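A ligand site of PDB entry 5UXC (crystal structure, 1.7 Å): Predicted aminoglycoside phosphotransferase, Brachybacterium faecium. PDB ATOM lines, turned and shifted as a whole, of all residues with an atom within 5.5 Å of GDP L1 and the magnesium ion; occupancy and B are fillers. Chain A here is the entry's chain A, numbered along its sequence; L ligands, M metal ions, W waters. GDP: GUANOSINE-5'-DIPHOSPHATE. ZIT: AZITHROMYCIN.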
ATOM      1  N   GLU A  28      22.999 -31.089   5.203  1.00  0.00           N
ATOM      2  CA  GLU A  28      23.547 -31.082   3.844  1.00  0.00           C
ATOM      3  C   GLU A  28      24.714 -30.113   3.682  1.00  0.00           C
ATOM      4  O   GLU A  28      25.740 -30.435   3.044  1.00  0.00           O
ATOM      5  CB  GLU A  28      22.419 -30.744   2.851  1.00  0.00           C
ATOM      6  CG  GLU A  28      22.841 -30.725   1.352  1.00  0.00           C
ATOM      7  CD  GLU A  28      23.363 -32.079   0.862  1.00  0.00           C
ATOM      8  OE1 GLU A  28      23.110 -33.124   1.527  1.00  0.00           O
ATOM      9  OE2 GLU A  28      24.050 -32.099  -0.208  1.00  0.00           O
ATOM     10  N   GLU A  29      24.604 -28.922   4.254  1.00  0.00           N
ATOM     11  CA  GLU A  29      25.595 -27.891   4.022  1.00  0.00           C
ATOM     12  C   GLU A  29      25.499 -26.879   5.154  1.00  0.00           C
ATOM     13  O   GLU A  29      24.399 -26.509   5.583  1.00  0.00           O
ATOM     14  CB  GLU A  29      25.371 -27.197   2.664  1.00  0.00           C
ATOM     15  CG  GLU A  29      26.387 -26.139   2.345  1.00  0.00           C
ATOM     16  CD  GLU A  29      26.340 -25.723   0.849  1.00  0.00           C
ATOM     17  OE1 GLU A  29      26.080 -24.533   0.575  1.00  0.00           O
ATOM     18  OE2 GLU A  29      26.604 -26.579  -0.031  1.00  0.00           O
ATOM     19  N   ILE A  30      26.629 -26.448   5.672  1.00  0.00           N
ATOM     20  CA  ILE A  30      26.648 -25.404   6.681  1.00  0.00           C
ATOM     21  C   ILE A  30      27.206 -24.153   6.036  1.00  0.00           C
ATOM     22  O   ILE A  30      28.423 -24.064   5.788  1.00  0.00           O
ATOM     23  CB  ILE A  30      27.464 -25.817   7.916  1.00  0.00           C
ATOM     24  CG1 ILE A  30      26.946 -27.190   8.405  1.00  0.00           C
ATOM     25  CG2 ILE A  30      27.401 -24.706   8.951  1.00  0.00           C
ATOM     26  CD1 ILE A  30      27.206 -27.456   9.855  1.00  0.00           C
ATOM     27  N   GLY A  31      26.323 -23.200   5.758  1.00  0.00           N
ATOM     28  CA  GLY A  31      26.704 -21.943   5.148  1.00  0.00           C
ATOM     29  C   GLY A  31      27.125 -20.908   6.176  1.00  0.00           C
ATOM     30  O   GLY A  31      27.104 -21.119   7.388  1.00  0.00           O
ATOM     31  N   PHE A  34      23.129 -19.819   7.035  1.00  0.00           N
ATOM     32  CA  PHE A  34      22.160 -20.878   7.296  1.00  0.00           C
ATOM     33  C   PHE A  34      22.820 -22.249   7.318  1.00  0.00           C
ATOM     34  O   PHE A  34      23.669 -22.559   6.467  1.00  0.00           O
ATOM     35  CB  PHE A  34      21.051 -20.882   6.243  1.00  0.00           C
ATOM     36  CG  PHE A  34      20.504 -19.523   5.923  1.00  0.00           C
ATOM     37  CD1 PHE A  34      21.138 -18.683   5.007  1.00  0.00           C
ATOM     38  CD2 PHE A  34      19.352 -19.076   6.541  1.00  0.00           C
ATOM     39  CE1 PHE A  34      20.620 -17.447   4.689  1.00  0.00           C
ATOM     40  CE2 PHE A  34      18.824 -17.828   6.248  1.00  0.00           C
ATOM     41  CZ  PHE A  34      19.470 -17.007   5.323  1.00  0.00           C
ATOM     42  N   VAL A  36      21.778 -25.902   6.412  1.00  0.00           N
ATOM     43  CA  VAL A  36      20.758 -26.459   5.519  1.00  0.00           C
ATOM     44  C   VAL A  36      20.737 -27.962   5.714  1.00  0.00           C
ATOM     45  O   VAL A  36      21.794 -28.593   5.732  1.00  0.00           O
ATOM     46  CB  VAL A  36      21.071 -26.107   4.051  1.00  0.00           C
ATOM     47  CG1 VAL A  36      20.008 -26.730   3.132  1.00  0.00           C
ATOM     48  CG2 VAL A  36      21.038 -24.615   3.885  1.00  0.00           C
ATOM     49  N   PHE A  38      18.256 -31.778   4.913  1.00  0.00           N
ATOM     50  CA  PHE A  38      17.181 -32.433   4.171  1.00  0.00           C
ATOM     51  C   PHE A  38      16.403 -33.303   5.147  1.00  0.00           C
ATOM     52  O   PHE A  38      16.999 -33.870   6.056  1.00  0.00           O
ATOM     53  CB  PHE A  38      17.715 -33.361   3.072  1.00  0.00           C
ATOM     54  CG  PHE A  38      18.354 -32.663   1.904  1.00  0.00           C
ATOM     55  CD1 PHE A  38      17.998 -31.398   1.580  1.00  0.00           C
ATOM     56  CD2 PHE A  38      19.299 -33.329   1.139  1.00  0.00           C
ATOM     57  CE1 PHE A  38      18.596 -30.780   0.461  1.00  0.00           C
ATOM     58  CE2 PHE A  38      19.899 -32.735   0.060  1.00  0.00           C
ATOM     59  CZ  PHE A  38      19.536 -31.482  -0.292  1.00  0.00           C
ATOM     60  N   VAL A  48      13.386 -29.300   2.691  1.00  0.00           N
ATOM     61  CA  VAL A  48      14.647 -28.638   3.007  1.00  0.00           C
ATOM     62  C   VAL A  48      14.418 -27.731   4.197  1.00  0.00           C
ATOM     63  O   VAL A  48      13.436 -26.965   4.222  1.00  0.00           O
ATOM     64  CB  VAL A  48      15.188 -27.810   1.823  1.00  0.00           C
ATOM     65  CG1 VAL A  48      16.531 -27.171   2.192  1.00  0.00           C
ATOM     66  CG2 VAL A  48      15.307 -28.646   0.595  1.00  0.00           C
ATOM     67  N   ARG A  50      16.107 -24.675   6.484  1.00  0.00           N
ATOM     68  CA  ARG A  50      17.131 -23.652   6.615  1.00  0.00           C
ATOM     69  C   ARG A  50      17.124 -23.145   8.052  1.00  0.00           C
ATOM     70  O   ARG A  50      16.110 -22.602   8.519  1.00  0.00           O
ATOM     71  CB  ARG A  50      16.889 -22.482   5.665  1.00  0.00           C
ATOM     72  CG  ARG A  50      16.981 -22.824   4.232  1.00  0.00           C
ATOM     73  CD  ARG A  50      16.778 -21.541   3.416  1.00  0.00           C
ATOM     74  NE  ARG A  50      17.936 -20.656   3.447  1.00  0.00           N
ATOM     75  CZ  ARG A  50      19.063 -20.895   2.784  1.00  0.00           C
ATOM     76  NH1 ARG A  50      20.068 -20.044   2.830  1.00  0.00           N
ATOM     77  NH2 ARG A  50      19.180 -21.990   2.068  1.00  0.00           N
ATOM     78  N   TYR A  92      11.086 -25.565   3.057  1.00  0.00           N
ATOM     79  CA  TYR A  92      10.424 -25.547   1.772  1.00  0.00           C
ATOM     80  C   TYR A  92      10.457 -26.950   1.220  1.00  0.00           C
ATOM     81  O   TYR A  92      11.378 -27.714   1.519  1.00  0.00           O
ATOM     82  CB  TYR A  92      11.061 -24.580   0.750  1.00  0.00           C
ATOM     83  CG  TYR A  92      12.550 -24.692   0.456  1.00  0.00           C
ATOM     84  CD1 TYR A  92      13.484 -23.931   1.186  1.00  0.00           C
ATOM     85  CD2 TYR A  92      13.014 -25.487  -0.611  1.00  0.00           C
ATOM     86  CE1 TYR A  92      14.877 -23.954   0.848  1.00  0.00           C
ATOM     87  CE2 TYR A  92      14.374 -25.520  -0.961  1.00  0.00           C
ATOM     88  CZ  TYR A  92      15.286 -24.735  -0.231  1.00  0.00           C
ATOM     89  OH  TYR A  92      16.647 -24.729  -0.565  1.00  0.00           O
ATOM     90  N   PRO A  93       9.446 -27.337   0.433  1.00  0.00           N
ATOM     91  CA  PRO A  93       9.488 -28.654  -0.218  1.00  0.00           C
ATOM     92  C   PRO A  93      10.714 -28.777  -1.099  1.00  0.00           C
ATOM     93  O   PRO A  93      11.113 -27.838  -1.809  1.00  0.00           O
ATOM     94  CB  PRO A  93       8.215 -28.685  -1.062  1.00  0.00           C
ATOM     95  CG  PRO A  93       7.250 -27.749  -0.249  1.00  0.00           C
ATOM     96  CD  PRO A  93       8.152 -26.635   0.232  1.00  0.00           C
ATOM     97  N   LEU A  94      11.313 -29.960  -1.030  1.00  0.00           N
ATOM     98  CA  LEU A  94      12.506 -30.254  -1.825  1.00  0.00           C
ATOM     99  C   LEU A  94      12.204 -30.096  -3.288  1.00  0.00           C
ATOM    100  O   LEU A  94      11.238 -30.673  -3.813  1.00  0.00           O
ATOM    101  CB  LEU A  94      12.938 -31.719  -1.537  1.00  0.00           C
ATOM    102  CG  LEU A  94      14.080 -32.124  -2.526  1.00  0.00           C
ATOM    103  CD1 LEU A  94      15.329 -31.819  -1.794  1.00  0.00           C
ATOM    104  CD2 LEU A  94      13.986 -33.605  -2.877  1.00  0.00           C
ATOM    105  N   LEU A  95      13.120 -29.250  -4.004  1.00  0.00           N
ATOM    106  CA  LEU A  95      12.869 -28.964  -5.391  1.00  0.00           C
ATOM    107  C   LEU A  95      13.482 -30.080  -6.251  1.00  0.00           C
ATOM    108  O   LEU A  95      14.480 -30.675  -5.864  1.00  0.00           O
ATOM    109  CB  LEU A  95      13.524 -27.619  -5.779  1.00  0.00           C
ATOM    110  CG  LEU A  95      12.845 -26.477  -4.999  1.00  0.00           C
ATOM    111  CD1 LEU A  95      13.655 -25.200  -5.111  1.00  0.00           C
ATOM    112  CD2 LEU A  95      11.427 -26.271  -5.514  1.00  0.00           C
ATOM    113  N   PRO A  96      12.880 -30.346  -7.401  1.00  0.00           N
ATOM    114  CA  PRO A  96      13.323 -31.498  -8.219  1.00  0.00           C
ATOM    115  C   PRO A  96      14.583 -31.174  -9.020  1.00  0.00           C
ATOM    116  O   PRO A  96      14.836 -30.016  -9.375  1.00  0.00           O
ATOM    117  CB  PRO A  96      12.141 -31.703  -9.166  1.00  0.00           C
ATOM    118  CG  PRO A  96      11.642 -30.325  -9.423  1.00  0.00           C
ATOM    119  CD  PRO A  96      11.771 -29.618  -8.038  1.00  0.00           C
ATOM    120  N   GLY A  97      15.300 -32.246  -9.368  1.00  0.00           N
ATOM    121  CA  GLY A  97      16.555 -32.149 -10.134  1.00  0.00           C
ATOM    122  C   GLY A  97      17.762 -32.353  -9.250  1.00  0.00           C
ATOM    123  O   GLY A  97      17.672 -32.516  -8.020  1.00  0.00           O
ATOM    124  N   SER A  98      18.921 -32.349  -9.894  1.00  0.00           N
ATOM    125  CA  SER A  98      20.177 -32.578  -9.215  1.00  0.00           C
ATOM    126  C   SER A  98      21.034 -31.326  -9.344  1.00  0.00           C
ATOM    127  O   SER A  98      21.047 -30.720 -10.402  1.00  0.00           O
ATOM    128  CB  SER A  98      20.990 -33.768  -9.826  1.00  0.00           C
ATOM    129  OG  SER A  98      20.197 -34.954  -9.944  1.00  0.00           O
ATOM    130  N   PRO A  99      21.738 -30.924  -8.292  1.00  0.00           N
ATOM    131  CA  PRO A  99      22.630 -29.752  -8.395  1.00  0.00           C
ATOM    132  C   PRO A  99      23.650 -29.965  -9.516  1.00  0.00           C
ATOM    133  O   PRO A  99      24.205 -31.065  -9.670  1.00  0.00           O
ATOM    134  CB  PRO A  99      23.313 -29.703  -7.030  1.00  0.00           C
ATOM    135  CG  PRO A  99      22.346 -30.476  -6.095  1.00  0.00           C
ATOM    136  CD  PRO A  99      21.767 -31.543  -6.956  1.00  0.00           C
ATOM    137  N   LEU A 101      26.592 -28.781  -9.756  1.00  0.00           N
ATOM    138  CA  LEU A 101      27.782 -29.255  -9.072  1.00  0.00           C
ATOM    139  C   LEU A 101      27.539 -29.201  -7.576  1.00  0.00           C
ATOM    140  O   LEU A 101      26.595 -28.551  -7.114  1.00  0.00           O
ATOM    141  CB  LEU A 101      29.033 -28.428  -9.474  1.00  0.00           C
ATOM    142  CG  LEU A 101      29.036 -26.929  -9.127  1.00  0.00           C
ATOM    143  CD1 LEU A 101      29.438 -26.730  -7.667  1.00  0.00           C
ATOM    144  CD2 LEU A 101      29.952 -26.075 -10.091  1.00  0.00           C
ATOM    145  N   THR A 102      28.380 -29.892  -6.809  1.00  0.00           N
ATOM    146  CA  THR A 102      28.307 -29.802  -5.355  1.00  0.00           C
ATOM    147  C   THR A 102      29.688 -29.548  -4.788  1.00  0.00           C
ATOM    148  O   THR A 102      30.665 -30.142  -5.239  1.00  0.00           O
ATOM    149  CB  THR A 102      27.661 -31.065  -4.753  1.00  0.00           C
ATOM    150  OG1 THR A 102      28.471 -32.197  -5.032  1.00  0.00           O
ATOM    151  CG2 THR A 102      26.313 -31.310  -5.402  1.00  0.00           C
ATOM    152  N   GLU A 197      24.465 -14.960  -7.251  1.00  0.00           N
ATOM    153  CA  GLU A 197      25.396 -16.062  -7.021  1.00  0.00           C
ATOM    154  C   GLU A 197      24.978 -17.222  -7.906  1.00  0.00           C
ATOM    155  O   GLU A 197      24.783 -18.356  -7.442  1.00  0.00           O
ATOM    156  CB  GLU A 197      25.445 -16.435  -5.539  1.00  0.00           C
ATOM    157  CG  GLU A 197      26.713 -17.172  -5.192  1.00  0.00           C
ATOM    158  CD  GLU A 197      26.991 -17.143  -3.719  1.00  0.00           C
ATOM    159  OE1 GLU A 197      27.199 -16.038  -3.160  1.00  0.00           O
ATOM    160  OE2 GLU A 197      26.967 -18.236  -3.139  1.00  0.00           O
ATOM    161  N   ALA A 201      26.020 -24.852  -8.560  1.00  0.00           N
ATOM    162  CA  ALA A 201      25.593 -25.340  -7.243  1.00  0.00           C
ATOM    163  C   ALA A 201      24.179 -24.902  -6.929  1.00  0.00           C
ATOM    164  O   ALA A 201      23.501 -25.513  -6.071  1.00  0.00           O
ATOM    165  CB  ALA A 201      26.489 -24.796  -6.136  1.00  0.00           C
ATOM    166  N   HIS A 202      23.742 -23.798  -7.532  1.00  0.00           N
ATOM    167  CA  HIS A 202      22.401 -23.301  -7.236  1.00  0.00           C
ATOM    168  C   HIS A 202      21.432 -23.492  -8.403  1.00  0.00           C
ATOM    169  O   HIS A 202      20.313 -22.977  -8.334  1.00  0.00           O
ATOM    170  CB  HIS A 202      22.481 -21.808  -6.803  1.00  0.00           C
ATOM    171  CG  HIS A 202      23.377 -21.548  -5.616  1.00  0.00           C
ATOM    172  ND1 HIS A 202      23.965 -20.323  -5.358  1.00  0.00           N
ATOM    173  CD2 HIS A 202      23.712 -22.337  -4.557  1.00  0.00           C
ATOM    174  CE1 HIS A 202      24.655 -20.384  -4.215  1.00  0.00           C
ATOM    175  NE2 HIS A 202      24.524 -21.596  -3.692  1.00  0.00           N
ATOM    176  N   LEU A 204      19.459 -26.557 -10.156  1.00  0.00           N
ATOM    177  CA  LEU A 204      19.187 -27.972 -10.279  1.00  0.00           C
ATOM    178  C   LEU A 204      18.865 -28.300 -11.727  1.00  0.00           C
ATOM    179  O   LEU A 204      18.203 -27.505 -12.422  1.00  0.00           O
ATOM    180  CB  LEU A 204      17.995 -28.368  -9.397  1.00  0.00           C
ATOM    181  CG  LEU A 204      18.090 -27.974  -7.933  1.00  0.00           C
ATOM    182  CD1 LEU A 204      16.881 -28.573  -7.131  1.00  0.00           C
ATOM    183  CD2 LEU A 204      19.414 -28.558  -7.325  1.00  0.00           C
ATOM    184  N   LEU A 214      18.159 -22.138  -6.758  1.00  0.00           N
ATOM    185  CA  LEU A 214      18.221 -22.100  -5.294  1.00  0.00           C
ATOM    186  C   LEU A 214      18.891 -20.822  -4.813  1.00  0.00           C
ATOM    187  O   LEU A 214      19.618 -20.170  -5.567  1.00  0.00           O
ATOM    188  CB  LEU A 214      19.049 -23.283  -4.742  1.00  0.00           C
ATOM    189  CG  LEU A 214      18.668 -24.645  -5.299  1.00  0.00           C
ATOM    190  CD1 LEU A 214      19.680 -25.711  -4.821  1.00  0.00           C
ATOM    191  CD2 LEU A 214      17.213 -24.998  -4.890  1.00  0.00           C
ATOM    192  N   ASP A 215      18.662 -20.489  -3.540  1.00  0.00           N
ATOM    193  CA  ASP A 215      19.547 -19.625  -2.717  1.00  0.00           C
ATOM    194  C   ASP A 215      19.559 -18.192  -3.215  1.00  0.00           C
ATOM    195  O   ASP A 215      20.545 -17.715  -3.833  1.00  0.00           O
ATOM    196  CB  ASP A 215      20.987 -20.190  -2.659  1.00  0.00           C
ATOM    197  CG  ASP A 215      21.859 -19.514  -1.577  1.00  0.00           C
ATOM    198  OD1 ASP A 215      21.259 -18.899  -0.702  1.00  0.00           O
ATOM    199  OD2 ASP A 215      23.102 -19.696  -1.474  1.00  0.00           O
HETATM  200  PB  GDP L   1      23.441 -21.999   1.731  1.00  0.00           P
HETATM  201  O1B GDP L   1      24.376 -21.728   0.586  1.00  0.00           O
HETATM  202  O2B GDP L   1      23.026 -20.814   2.484  1.00  0.00           O
HETATM  203  O3B GDP L   1      24.203 -23.046   2.649  1.00  0.00           O
HETATM  204  O3A GDP L   1      22.099 -22.684   1.173  1.00  0.00           O
HETATM  205  PA  GDP L   1      21.636 -23.243  -0.241  1.00  0.00           P
HETATM  206  O1A GDP L   1      20.235 -22.735  -0.372  1.00  0.00           O
HETATM  207  O2A GDP L   1      22.607 -22.897  -1.349  1.00  0.00           O
HETATM  208  O5' GDP L   1      21.527 -24.823  -0.115  1.00  0.00           O
HETATM  209  C5' GDP L   1      22.747 -25.531   0.125  1.00  0.00           C
HETATM  210  C4' GDP L   1      22.869 -26.703  -0.818  1.00  0.00           C
HETATM  211  O4' GDP L   1      21.813 -27.614  -0.522  1.00  0.00           O
HETATM  212  C3' GDP L   1      22.642 -26.318  -2.281  1.00  0.00           C
HETATM  213  O3' GDP L   1      23.805 -25.824  -2.987  1.00  0.00           O
HETATM  214  C2' GDP L   1      22.201 -27.627  -2.871  1.00  0.00           C
HETATM  215  O2' GDP L   1      23.315 -28.554  -2.993  1.00  0.00           O
HETATM  216  C1' GDP L   1      21.354 -28.211  -1.727  1.00  0.00           C
HETATM  217  N9  GDP L   1      19.909 -27.842  -1.850  1.00  0.00           N
HETATM  218  C8  GDP L   1      19.286 -26.795  -1.293  1.00  0.00           C
HETATM  219  N7  GDP L   1      17.953 -26.824  -1.625  1.00  0.00           N
HETATM  220  C5  GDP L   1      17.774 -27.902  -2.424  1.00  0.00           C
HETATM  221  C6  GDP L   1      16.685 -28.549  -3.148  1.00  0.00           C
HETATM  222  O6  GDP L   1      15.523 -28.091  -3.070  1.00  0.00           O
HETATM  223  N1  GDP L   1      16.930 -29.685  -3.843  1.00  0.00           N
HETATM  224  C2  GDP L   1      18.162 -30.241  -3.908  1.00  0.00           C
HETATM  225  N2  GDP L   1      18.322 -31.370  -4.619  1.00  0.00           N
HETATM  226  N3  GDP L   1      19.235 -29.705  -3.307  1.00  0.00           N
HETATM  227  C4  GDP L   1      19.092 -28.552  -2.583  1.00  0.00           C
HETATM  228  C1  ZIT L   2      17.231 -36.957  -0.041  1.00  0.00           C
HETATM  229  C2  ZIT L   2      18.156 -36.214  -1.052  1.00  0.00           C
HETATM  230  C3  ZIT L   2      18.662 -37.271  -1.998  1.00  0.00           C
HETATM  231  C4  ZIT L   2      20.140 -37.503  -1.629  1.00  0.00           C
HETATM  232  C5  ZIT L   2      20.534 -38.812  -2.358  1.00  0.00           C
HETATM  233  C6  ZIT L   2      21.022 -39.902  -1.393  1.00  0.00           C
HETATM  234  C7  ZIT L   2      22.068 -39.410  -0.355  1.00  0.00           C
HETATM  235  C8  ZIT L   2      22.424 -40.574   0.651  1.00  0.00           C
HETATM  236  C9  ZIT L   2      21.383 -40.831   1.805  1.00  0.00           C
HETATM  237  N10 ZIT L   2      20.833 -39.563   2.528  1.00  0.00           N
HETATM  238  C11 ZIT L   2      19.586 -39.725   3.248  1.00  0.00           C
HETATM  239  C12 ZIT L   2      18.434 -39.169   2.434  1.00  0.00           C
HETATM  240  C13 ZIT L   2      17.632 -38.140   3.217  1.00  0.00           C
HETATM  241  C14 ZIT L   2      16.673 -37.485   2.240  1.00  0.00           C
HETATM  242  C15 ZIT L   2      15.702 -36.547   2.936  1.00  0.00           C
HETATM  243  C16 ZIT L   2      14.677 -36.046   1.855  1.00  0.00           C
HETATM  244  C17 ZIT L   2      17.410 -35.055  -1.644  1.00  0.00           C
HETATM  245  C18 ZIT L   2      20.926 -36.265  -1.985  1.00  0.00           C
HETATM  246  C19 ZIT L   2      21.533 -41.180  -2.071  1.00  0.00           C
HETATM  247  C20 ZIT L   2      23.786 -40.347   1.153  1.00  0.00           C
HETATM  248  C21 ZIT L   2      21.768 -39.090   3.544  1.00  0.00           C
HETATM  249  C22 ZIT L   2      19.314 -41.169   3.616  1.00  0.00           C
HETATM  250  C23 ZIT L   2      18.574 -37.101   3.826  1.00  0.00           C
HETATM  251  O1  ZIT L   2      16.389 -37.745  -0.425  1.00  0.00           O
HETATM  252  O6  ZIT L   2      19.840 -40.246  -0.699  1.00  0.00           O
HETATM  253  O12 ZIT L   2      17.570 -40.209   2.071  1.00  0.00           O
HETATM  254  O13 ZIT L   2      16.905 -38.796   4.284  1.00  0.00           O
HETATM  255  O14 ZIT L   2      17.482 -36.660   1.392  1.00  0.00           O
HETATM  256  C1A ZIT L   2      22.447 -38.706  -4.058  1.00  0.00           C
HETATM  257  C2A ZIT L   2      22.349 -38.587  -5.567  1.00  0.00           C
HETATM  258  C3A ZIT L   2      23.584 -38.067  -6.228  1.00  0.00           C
HETATM  259  C4A ZIT L   2      24.028 -36.849  -5.544  1.00  0.00           C
HETATM  260  C5A ZIT L   2      24.382 -37.195  -4.108  1.00  0.00           C
HETATM  261  C6A ZIT L   2      24.953 -36.033  -3.409  1.00  0.00           C
HETATM  262  C7A ZIT L   2      24.236 -36.762  -8.172  1.00  0.00           C
HETATM  263  C8A ZIT L   2      23.595 -39.009  -8.482  1.00  0.00           C
HETATM  264  O1A ZIT L   2      21.108 -38.588  -3.652  1.00  0.00           O
HETATM  265  O2A ZIT L   2      21.975 -39.865  -6.084  1.00  0.00           O
HETATM  266  N3A ZIT L   2      23.354 -37.795  -7.674  1.00  0.00           N
HETATM  267  O5A ZIT L   2      23.202 -37.666  -3.366  1.00  0.00           O
HETATM  268  C1B ZIT L   2      17.377 -37.396  -4.034  1.00  0.00           C
HETATM  269  C2B ZIT L   2      17.094 -36.560  -5.251  1.00  0.00           C
HETATM  270  C3B ZIT L   2      17.970 -36.900  -6.427  1.00  0.00           C
HETATM  271  C4B ZIT L   2      18.002 -38.376  -6.663  1.00  0.00           C
HETATM  272  C5B ZIT L   2      18.457 -39.115  -5.432  1.00  0.00           C
HETATM  273  C6B ZIT L   2      18.458 -40.602  -5.692  1.00  0.00           C
HETATM  274  C7B ZIT L   2      17.468 -36.170  -7.731  1.00  0.00           C
HETATM  275  C8B ZIT L   2      19.568 -35.094  -6.001  1.00  0.00           C
HETATM  276  O1B ZIT L   2      18.519 -36.903  -3.386  1.00  0.00           O
HETATM  277  O3B ZIT L   2      19.304 -36.476  -6.149  1.00  0.00           O
HETATM  278  O4B ZIT L   2      18.916 -38.682  -7.736  1.00  0.00           O
HETATM  279  O5B ZIT L   2      17.572 -38.851  -4.310  1.00  0.00           O
HETATM  280 MG    MG M   1      24.106 -21.567  -1.590  1.00  0.00          MG
HETATM  281  O   HOH W   1      27.170 -22.038   1.134  1.00  0.00           O
HETATM  282  O   HOH W   2      25.181 -27.655  -4.824  1.00  0.00           O
HETATM  283  O   HOH W   3      20.907 -32.694  -3.846  1.00  0.00           O
HETATM  284  O   HOH W   4      17.806 -22.422  -1.424  1.00  0.00           O
HETATM  285  O   HOH W   5      22.846 -18.347   1.450  1.00  0.00           O
HETATM  286  O   HOH W   6      24.136 -19.476   4.526  1.00  0.00           O
HETATM  287  O   HOH W   7      25.360 -23.348  -1.700  1.00  0.00           O
HETATM  288  O   HOH W   8      16.046 -32.718  -5.886  1.00  0.00           O
HETATM  289  O   HOH W   9      22.994 -31.360  -2.551  1.00  0.00           O
HETATM  290  O   HOH W  10      25.732 -20.281  -1.390  1.00  0.00           O
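An oxygen (O6) of GDP L1 lies within hydrogen-bond range of the backbone NH (N) of Leu 95.
O of Ala 201 is in hydrogen-bond range of O3' of GDP L1 (3.1 Å).
The side-chain hydroxyl of Tyr 92 lies within hydrogen-bond range of a nitrogen (N7) of GDP L1, 2.7 Å away.
The backbone carbonyl oxygen (O) of Leu 95 is in hydrogen-bond range of a nitrogen (N1) of GDP L1 (3.3 Å).
NH2 of Arg 50 is in salt-bridge range of O1A of GDP L1 (2.8 Å).
N of Val 36 sits at hydrogen-bond distance from O of Glu 29 (2.8 Å).
N of Glu 28 is in hydrogen-bond range of O of Val 36, 2.8 Å away.
The backbone carbonyl oxygen of Glu 197 sits at hydrogen-bond distance from a ring nitrogen (ND1) of His 202 (3.0 Å).
N of Val 48 sits at hydrogen-bond distance from O of Tyr 92, at 2.8 Å.
OD1 of Asp 215 lies within salt-bridge range of NH1 of Arg 50 (3.9 Å).
The backbone NH of Leu 214 sits at hydrogen-bond distance from the backbone carbonyl oxygen of His 202, 2.8 Å away.
OE1 of Glu 29 lies close to O3B of GDP L1 (3.2 Å).
Merely in contact with GDP L1: Leu 94, Leu 204, Val 36, Phe 38, Gly 97, Leu 214, Gly 31, Val 48, Glu 28, Pro 99 and Phe 34.
The nearest printed residue that does not touch GDP L1 is Pro 93 (4.6 Å).
Of the 25 residues printed, 2 come within 4 Å of the magnesium ion.
The magnesium ion is bound by an oxygen (O2A) of GDP L1 (2.0 Å), water W10 (2.1 Å), the side-chain carboxylate (OD2) of Asp 215 (2.1 Å), a ring nitrogen (NE2) of His 202 (2.1 Å), water W7 (2.2 Å) and an oxygen (O1B) of GDP L1 (2.2 Å).
Water W7 bridges OE1 of Glu 29 (2.7 Å) and O3' of GDP L1 (3.2 Å).
Water W4 lies within hydrogen-bond range of O1A of GDP L1 (2.7 Å), OH of Tyr 92 (2.7 Å) and N of Asp 215 (3.0 Å).
Water W5 lies within hydrogen-bond range of an oxygen (O2B) of GDP L1 and the side-chain carboxylate (OD1) of Asp 215.
Water W2 lies within hydrogen-bond range of an oxygen (O2') of GDP L1 (2.8 Å), the backbone carbonyl oxygen of Leu 101 (2.8 Å) and the backbone carbonyl oxygen of Ala 201 (3.0 Å).
Water W9 bridges OE2 of Glu 28 (2.7 Å) and O2' of GDP L1 (2.9 Å).
Water W8 lies within hydrogen-bond range of O of Leu 95 (2.6 Å), O of Gly 97 (2.7 Å) and N2 of GDP L1 (2.9 Å).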
